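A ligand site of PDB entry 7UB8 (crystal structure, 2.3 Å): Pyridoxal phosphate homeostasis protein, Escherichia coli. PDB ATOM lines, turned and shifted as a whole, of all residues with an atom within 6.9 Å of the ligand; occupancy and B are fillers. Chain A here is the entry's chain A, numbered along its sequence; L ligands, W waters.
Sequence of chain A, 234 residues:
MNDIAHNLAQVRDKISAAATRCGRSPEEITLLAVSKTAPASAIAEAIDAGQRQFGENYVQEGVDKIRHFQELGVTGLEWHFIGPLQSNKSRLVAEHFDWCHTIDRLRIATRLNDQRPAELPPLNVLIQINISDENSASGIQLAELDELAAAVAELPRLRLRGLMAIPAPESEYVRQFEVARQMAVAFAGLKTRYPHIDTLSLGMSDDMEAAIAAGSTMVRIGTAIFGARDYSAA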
ATOM      1  N   LEU A  32     -34.745   5.805  -7.143  1.00  0.00           N
ATOM      2  CA  LEU A  32     -33.589   6.486  -7.716  1.00  0.00           C
ATOM      3  C   LEU A  32     -33.602   6.149  -9.195  1.00  0.00           C
ATOM      4  O   LEU A  32     -33.399   4.986  -9.564  1.00  0.00           O
ATOM      5  CB  LEU A  32     -32.275   6.075  -7.053  1.00  0.00           C
ATOM      6  CG  LEU A  32     -31.047   6.764  -7.666  1.00  0.00           C
ATOM      7  CD1 LEU A  32     -31.033   8.268  -7.333  1.00  0.00           C
ATOM      8  CD2 LEU A  32     -29.744   6.090  -7.225  1.00  0.00           C
ATOM      9  N   VAL A  34     -32.061   5.798 -12.491  1.00  0.00           N
ATOM     10  CA  VAL A  34     -30.701   5.663 -12.951  1.00  0.00           C
ATOM     11  C   VAL A  34     -30.657   6.084 -14.401  1.00  0.00           C
ATOM     12  O   VAL A  34     -31.246   5.437 -15.277  1.00  0.00           O
ATOM     13  CB  VAL A  34     -30.186   4.224 -12.764  1.00  0.00           C
ATOM     14  CG1 VAL A  34     -28.759   4.136 -13.315  1.00  0.00           C
ATOM     15  CG2 VAL A  34     -30.226   3.853 -11.317  1.00  0.00           C
ATOM     16  N   LYS A  36     -27.674   6.815 -16.201  1.00  0.00           N
ATOM     17  CA  LYS A  36     -26.460   6.516 -16.951  1.00  0.00           C
ATOM     18  C   LYS A  36     -26.852   6.005 -18.338  1.00  0.00           C
ATOM     19  O   LYS A  36     -27.786   5.208 -18.483  1.00  0.00           O
ATOM     20  CB  LYS A  36     -25.591   5.480 -16.205  1.00  0.00           C
ATOM     21  CG  LYS A  36     -26.155   4.041 -16.161  1.00  0.00           C
ATOM     22  CD  LYS A  36     -25.050   3.029 -16.492  1.00  0.00           C
ATOM     23  CE  LYS A  36     -25.502   1.587 -16.291  1.00  0.00           C
ATOM     24  NZ  LYS A  36     -25.938   1.280 -14.899  1.00  0.00           N
ATOM     25  N   ASN A  57     -23.386   7.002 -13.192  1.00  0.00           N
ATOM     26  CA  ASN A  57     -22.265   6.094 -12.994  1.00  0.00           C
ATOM     27  C   ASN A  57     -20.923   6.655 -13.454  1.00  0.00           C
ATOM     28  O   ASN A  57     -19.885   6.245 -12.910  1.00  0.00           O
ATOM     29  CB  ASN A  57     -22.507   4.778 -13.728  1.00  0.00           C
ATOM     30  CG  ASN A  57     -23.599   3.976 -13.099  1.00  0.00           C
ATOM     31  OD1 ASN A  57     -24.781   4.358 -13.141  1.00  0.00           O
ATOM     32  ND2 ASN A  57     -23.224   2.827 -12.502  1.00  0.00           N
ATOM     33  N   TYR A  58     -20.895   7.542 -14.434  1.00  0.00           N
ATOM     34  CA  TYR A  58     -19.656   8.020 -15.030  1.00  0.00           C
ATOM     35  C   TYR A  58     -19.524   9.516 -14.752  1.00  0.00           C
ATOM     36  O   TYR A  58     -20.410  10.290 -15.114  1.00  0.00           O
ATOM     37  CB  TYR A  58     -19.633   7.743 -16.535  1.00  0.00           C
ATOM     38  CG  TYR A  58     -20.160   6.359 -16.901  1.00  0.00           C
ATOM     39  CD1 TYR A  58     -19.392   5.214 -16.663  1.00  0.00           C
ATOM     40  CD2 TYR A  58     -21.408   6.201 -17.483  1.00  0.00           C
ATOM     41  CE1 TYR A  58     -19.868   3.953 -16.999  1.00  0.00           C
ATOM     42  CE2 TYR A  58     -21.884   4.949 -17.839  1.00  0.00           C
ATOM     43  CZ  TYR A  58     -21.107   3.824 -17.583  1.00  0.00           C
ATOM     44  OH  TYR A  58     -21.592   2.575 -17.928  1.00  0.00           O
ATOM     45  N   ILE A  82     -23.225   6.651  -8.424  1.00  0.00           N
ATOM     46  CA  ILE A  82     -23.413   5.257  -8.064  1.00  0.00           C
ATOM     47  C   ILE A  82     -22.447   4.352  -8.805  1.00  0.00           C
ATOM     48  O   ILE A  82     -22.587   3.122  -8.748  1.00  0.00           O
ATOM     49  CB  ILE A  82     -24.878   4.821  -8.308  1.00  0.00           C
ATOM     50  CG1 ILE A  82     -25.188   4.823  -9.803  1.00  0.00           C
ATOM     51  CG2 ILE A  82     -25.832   5.764  -7.560  1.00  0.00           C
ATOM     52  CD1 ILE A  82     -26.551   4.235 -10.135  1.00  0.00           C
ATOM     53  N   GLY A  83     -21.476   4.923  -9.513  1.00  0.00           N
ATOM     54  CA  GLY A  83     -20.430   4.178 -10.168  1.00  0.00           C
ATOM     55  C   GLY A  83     -19.172   4.132  -9.309  1.00  0.00           C
ATOM     56  O   GLY A  83     -19.057   4.836  -8.308  1.00  0.00           O
ATOM     57  N   THR A 102     -20.744   4.719  -3.307  1.00  0.00           N
ATOM     58  CA  THR A 102     -19.715   3.721  -3.599  1.00  0.00           C
ATOM     59  C   THR A 102     -18.451   3.903  -2.748  1.00  0.00           C
ATOM     60  O   THR A 102     -17.335   3.663  -3.215  1.00  0.00           O
ATOM     61  CB  THR A 102     -19.399   3.735  -5.078  1.00  0.00           C
ATOM     62  OG1 THR A 102     -19.073   5.075  -5.472  1.00  0.00           O
ATOM     63  CG2 THR A 102     -20.617   3.272  -5.874  1.00  0.00           C
ATOM     64  N   GLN A 128     -20.372   0.820   0.362  1.00  0.00           N
ATOM     65  CA  GLN A 128     -20.729  -0.256  -0.558  1.00  0.00           C
ATOM     66  C   GLN A 128     -20.205  -1.603  -0.063  1.00  0.00           C
ATOM     67  O   GLN A 128     -19.012  -1.753   0.213  1.00  0.00           O
ATOM     68  CB  GLN A 128     -20.204   0.036  -1.960  1.00  0.00           C
ATOM     69  CG  GLN A 128     -20.498  -1.066  -2.997  1.00  0.00           C
ATOM     70  CD  GLN A 128     -20.096  -0.656  -4.419  1.00  0.00           C
ATOM     71  OE1 GLN A 128     -19.472   0.388  -4.618  1.00  0.00           O
ATOM     72  NE2 GLN A 128     -20.471  -1.458  -5.406  1.00  0.00           N
ATOM     73  N   MET A 164     -24.994   0.390   0.464  1.00  0.00           N
ATOM     74  CA  MET A 164     -25.337   0.075  -0.916  1.00  0.00           C
ATOM     75  C   MET A 164     -24.727  -1.273  -1.277  1.00  0.00           C
ATOM     76  O   MET A 164     -23.652  -1.613  -0.780  1.00  0.00           O
ATOM     77  CB  MET A 164     -24.814   1.160  -1.880  1.00  0.00           C
ATOM     78  CG  MET A 164     -25.274   1.064  -3.313  1.00  0.00           C
ATOM     79  SD  MET A 164     -24.377  -0.092  -4.370  1.00  0.00           S
ATOM     80  CE  MET A 164     -23.085   0.898  -5.040  1.00  0.00           C
ATOM     81  N   ALA A 165     -25.410  -2.035  -2.108  1.00  0.00           N
ATOM     82  CA  ALA A 165     -24.799  -3.239  -2.666  1.00  0.00           C
ATOM     83  C   ALA A 165     -25.285  -3.462  -4.082  1.00  0.00           C
ATOM     84  O   ALA A 165     -26.425  -3.145  -4.430  1.00  0.00           O
ATOM     85  CB  ALA A 165     -25.086  -4.499  -1.845  1.00  0.00           C
ATOM     86  N   ILE A 166     -24.398  -4.014  -4.905  1.00  0.00           N
ATOM     87  CA  ILE A 166     -24.801  -4.597  -6.179  1.00  0.00           C
ATOM     88  C   ILE A 166     -24.557  -6.097  -6.089  1.00  0.00           C
ATOM     89  O   ILE A 166     -23.438  -6.567  -6.368  1.00  0.00           O
ATOM     90  CB  ILE A 166     -24.024  -3.979  -7.349  1.00  0.00           C
ATOM     91  CG1 ILE A 166     -24.187  -2.455  -7.349  1.00  0.00           C
ATOM     92  CG2 ILE A 166     -24.495  -4.574  -8.644  1.00  0.00           C
ATOM     93  CD1 ILE A 166     -23.023  -1.718  -8.005  1.00  0.00           C
ATOM     94  N   SER A 201     -29.449   1.251  -0.181  1.00  0.00           N
ATOM     95  CA  SER A 201     -29.570   1.345  -1.641  1.00  0.00           C
ATOM     96  C   SER A 201     -29.420  -0.057  -2.208  1.00  0.00           C
ATOM     97  O   SER A 201     -28.310  -0.584  -2.313  1.00  0.00           O
ATOM     98  CB  SER A 201     -28.513   2.309  -2.191  1.00  0.00           C
ATOM     99  OG  SER A 201     -28.434   2.252  -3.609  1.00  0.00           O
ATOM    100  N   GLY A 203     -31.444  -3.136  -4.859  1.00  0.00           N
ATOM    101  CA  GLY A 203     -32.458  -3.534  -5.803  1.00  0.00           C
ATOM    102  C   GLY A 203     -32.433  -2.751  -7.101  1.00  0.00           C
ATOM    103  O   GLY A 203     -32.350  -1.512  -7.121  1.00  0.00           O
ATOM    104  N   MET A 204     -32.486  -3.490  -8.200  1.00  0.00           N
ATOM    105  CA  MET A 204     -32.586  -2.956  -9.555  1.00  0.00           C
ATOM    106  C   MET A 204     -33.863  -3.528 -10.201  1.00  0.00           C
ATOM    107  O   MET A 204     -34.699  -4.131  -9.517  1.00  0.00           O
ATOM    108  CB  MET A 204     -31.310  -3.287 -10.332  1.00  0.00           C
ATOM    109  CG  MET A 204     -30.049  -2.592  -9.789  1.00  0.00           C
ATOM    110  SD  MET A 204     -28.567  -3.277 -10.568  1.00  0.00           S
ATOM    111  CE  MET A 204     -27.218  -2.496  -9.757  1.00  0.00           C
ATOM    112  N   SER A 205     -34.003  -3.346 -11.520  1.00  0.00           N
ATOM    113  CA  SER A 205     -35.270  -3.671 -12.184  1.00  0.00           C
ATOM    114  C   SER A 205     -35.663  -5.129 -11.979  1.00  0.00           C
ATOM    115  O   SER A 205     -36.828  -5.430 -11.690  1.00  0.00           O
ATOM    116  CB  SER A 205     -35.200  -3.355 -13.684  1.00  0.00           C
ATOM    117  OG  SER A 205     -35.221  -1.964 -13.938  1.00  0.00           O
ATOM    118  N   ASP A 206     -34.708  -6.042 -12.124  1.00  0.00           N
ATOM    119  CA  ASP A 206     -34.950  -7.477 -12.140  1.00  0.00           C
ATOM    120  C   ASP A 206     -35.130  -8.082 -10.748  1.00  0.00           C
ATOM    121  O   ASP A 206     -35.580  -9.238 -10.657  1.00  0.00           O
ATOM    122  CB  ASP A 206     -33.798  -8.204 -12.838  1.00  0.00           C
ATOM    123  CG  ASP A 206     -33.766  -7.940 -14.342  1.00  0.00           C
ATOM    124  OD1 ASP A 206     -34.747  -7.380 -14.887  1.00  0.00           O
ATOM    125  OD2 ASP A 206     -32.739  -8.279 -14.967  1.00  0.00           O
ATOM    126  N   VAL A 219     -34.561   1.730  -4.413  1.00  0.00           N
ATOM    127  CA  VAL A 219     -34.269   0.904  -5.580  1.00  0.00           C
ATOM    128  C   VAL A 219     -33.728   1.796  -6.691  1.00  0.00           C
ATOM    129  O   VAL A 219     -34.134   2.954  -6.831  1.00  0.00           O
ATOM    130  CB  VAL A 219     -35.524   0.129  -6.040  1.00  0.00           C
ATOM    131  CG1 VAL A 219     -35.895  -0.902  -4.995  1.00  0.00           C
ATOM    132  CG2 VAL A 219     -36.698   1.091  -6.294  1.00  0.00           C
ATOM    133  N   ARG A 220     -32.800   1.256  -7.470  1.00  0.00           N
ATOM    134  CA  ARG A 220     -32.052   1.999  -8.480  1.00  0.00           C
ATOM    135  C   ARG A 220     -32.506   1.447  -9.828  1.00  0.00           C
ATOM    136  O   ARG A 220     -32.057   0.384 -10.250  1.00  0.00           O
ATOM    137  CB  ARG A 220     -30.551   1.823  -8.300  1.00  0.00           C
ATOM    138  CG  ARG A 220     -29.977   2.215  -6.941  1.00  0.00           C
ATOM    139  CD  ARG A 220     -28.441   2.088  -6.968  1.00  0.00           C
ATOM    140  NE  ARG A 220     -28.062   0.732  -7.393  1.00  0.00           N
ATOM    141  CZ  ARG A 220     -28.033  -0.320  -6.576  1.00  0.00           C
ATOM    142  NH1 ARG A 220     -28.332  -0.174  -5.296  1.00  0.00           N
ATOM    143  NH2 ARG A 220     -27.711  -1.504  -7.040  1.00  0.00           N
ATOM    144  N   ILE A 221     -33.405   2.174 -10.480  1.00  0.00           N
ATOM    145  CA  ILE A 221     -34.078   1.677 -11.674  1.00  0.00           C
ATOM    146  C   ILE A 221     -33.605   2.479 -12.874  1.00  0.00           C
ATOM    147  O   ILE A 221     -33.781   3.700 -12.913  1.00  0.00           O
ATOM    148  CB  ILE A 221     -35.609   1.747 -11.544  1.00  0.00           C
ATOM    149  CG1 ILE A 221     -36.057   0.949 -10.326  1.00  0.00           C
ATOM    150  CG2 ILE A 221     -36.270   1.210 -12.808  1.00  0.00           C
ATOM    151  CD1 ILE A 221     -35.547  -0.493 -10.370  1.00  0.00           C
ATOM    152  N   GLY A 222     -33.018   1.787 -13.839  1.00  0.00           N
ATOM    153  CA  GLY A 222     -32.601   2.416 -15.058  1.00  0.00           C
ATOM    154  C   GLY A 222     -33.515   2.078 -16.217  1.00  0.00           C
ATOM    155  O   GLY A 222     -34.396   2.870 -16.591  1.00  0.00           O
ATOM    156  N   THR A 223     -33.348   0.861 -16.752  1.00  0.00           N
ATOM    157  CA  THR A 223     -33.915   0.503 -18.053  1.00  0.00           C
ATOM    158  C   THR A 223     -35.450   0.503 -18.042  1.00  0.00           C
ATOM    159  O   THR A 223     -36.080   0.919 -19.008  1.00  0.00           O
ATOM    160  CB  THR A 223     -33.359  -0.854 -18.489  1.00  0.00           C
ATOM    161  OG1 THR A 223     -31.995  -0.684 -18.899  1.00  0.00           O
ATOM    162  CG2 THR A 223     -34.171  -1.443 -19.642  1.00  0.00           C
ATOM    163  N   ALA A 224     -36.058   0.081 -16.938  1.00  0.00           N
ATOM    164  CA  ALA A 224     -37.507   0.115 -16.816  1.00  0.00           C
ATOM    165  C   ALA A 224     -38.071   1.538 -16.835  1.00  0.00           C
ATOM    166  O   ALA A 224     -39.300   1.694 -16.875  1.00  0.00           O
ATOM    167  CB  ALA A 224     -37.944  -0.599 -15.542  1.00  0.00           C
ATOM    168  N   ILE A 225     -37.224   2.564 -16.778  1.00  0.00           N
ATOM    169  CA  ILE A 225     -37.662   3.953 -16.892  1.00  0.00           C
ATOM    170  C   ILE A 225     -37.278   4.552 -18.237  1.00  0.00           C
ATOM    171  O   ILE A 225     -38.110   5.141 -18.932  1.00  0.00           O
ATOM    172  CB  ILE A 225     -37.114   4.810 -15.725  1.00  0.00           C
ATOM    173  CG1 ILE A 225     -37.845   4.469 -14.428  1.00  0.00           C
ATOM    174  CG2 ILE A 225     -37.239   6.300 -16.051  1.00  0.00           C
ATOM    175  CD1 ILE A 225     -37.224   5.057 -13.191  1.00  0.00           C
HETATM  176  N1  LIG L   1     -27.608   0.569 -10.092  1.00  0.00           N
HETATM  177  C1  LIG L   1     -26.329   0.633 -10.599  1.00  0.00           C
HETATM  178  C2  LIG L   1     -25.173   0.698  -9.631  1.00  0.00           C
HETATM  179  C3  LIG L   1     -26.137   0.618 -11.972  1.00  0.00           C
HETATM  180  O1  LIG L   1     -24.872   0.698 -12.458  1.00  0.00           O
HETATM  181  C4  LIG L   1     -27.244   0.544 -12.845  1.00  0.00           C
HETATM  182  C5  LIG L   1     -27.092   0.775 -14.322  1.00  0.00           C
HETATM  183  C6  LIG L   1     -28.525   0.494 -12.308  1.00  0.00           C
HETATM  184  C7  LIG L   1     -28.680   0.498 -10.939  1.00  0.00           C
HETATM  185  C8  LIG L   1     -29.763   0.398 -13.164  1.00  0.00           C
HETATM  186  O2  LIG L   1     -29.756  -0.825 -13.892  1.00  0.00           O
HETATM  187  P1  LIG L   1     -31.079  -1.370 -14.653  1.00  0.00           P
HETATM  188  O3  LIG L   1     -30.934  -2.855 -14.935  1.00  0.00           O
HETATM  189  O4  LIG L   1     -32.308  -1.162 -13.778  1.00  0.00           O
HETATM  190  O5  LIG L   1     -31.173  -0.658 -15.975  1.00  0.00           O
HETATM  191  O   HOH W   1     -29.288   1.083 -16.992  1.00  0.00           O
HETATM  192  O   HOH W   2     -31.928  -5.115 -13.161  1.00  0.00           O
HETATM  193  O   HOH W   3     -22.464  -0.515 -11.849  1.00  0.00           O
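Water W3 lies within hydrogen-bond range of O1 of the ligand (2.8 Å) and ND2 of Asn 57 (3.5 Å).
Water W2 lies within hydrogen-bond range of O3 of the ligand (3.0 Å), N of Asp 206 (3.1 Å) and N of Ser 205 (3.2 Å).
The backbone NH (N) of Arg 220 lies within hydrogen-bond range of the backbone carbonyl oxygen (O) of Gly 203 (2.8 Å).
The backbone carbonyl oxygen (O) of Ala 165 lies within hydrogen-bond range of the guanidinium group (NH2) of Arg 220, at 3.3 Å.
The side-chain hydroxyl of Ser 201 lies within hydrogen-bond range of the guanidinium group of Arg 220, at 3.0 Å.
The backbone NH of Val 34 lies within hydrogen-bond range of the backbone carbonyl oxygen of Ile 221, at 2.7 Å.
The backbone carbonyl oxygen (O) of Leu 32 sits at hydrogen-bond distance from the backbone NH (N) of Ile 221 (3.0 Å).
A carbon (C5) of the ligand is bonded to the side-chain amino group (NZ) of Lys 36, 1.4 Å away.
O1 of the ligand sits at hydrogen-bond distance from ND2 of Asn 57.
A nitrogen (N1) of the ligand sits at hydrogen-bond distance from the guanidinium group (NE) of Arg 220 (2.7 Å).
N of Thr 223 lies within hydrogen-bond range of O5 of the ligand, 2.8 Å away.
The side-chain hydroxyl of Thr 223 sits at hydrogen-bond distance from an oxygen (O5) of the ligand.
The side-chain hydroxyl of Ser 205 lies within hydrogen-bond range of an oxygen (O4) of the ligand (3.0 Å).
The backbone NH (N) of Gly 222 lies within hydrogen-bond range of an oxygen (O4) of the ligand.
Merely in contact with the ligand: Val 34 (3.7 Å), Ile 82 (3.6 Å), Ile 166 (3.6 Å), Met 204 (3.1 Å) and Ile 221 (3.95 Å).
Hydrophobic or aromatic side chains that line the ligand: Val 34, Ile 82, Ile 166 and Met 204.
Along chain A the residues within 4 Å of the ligand span positions 34 to 223.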
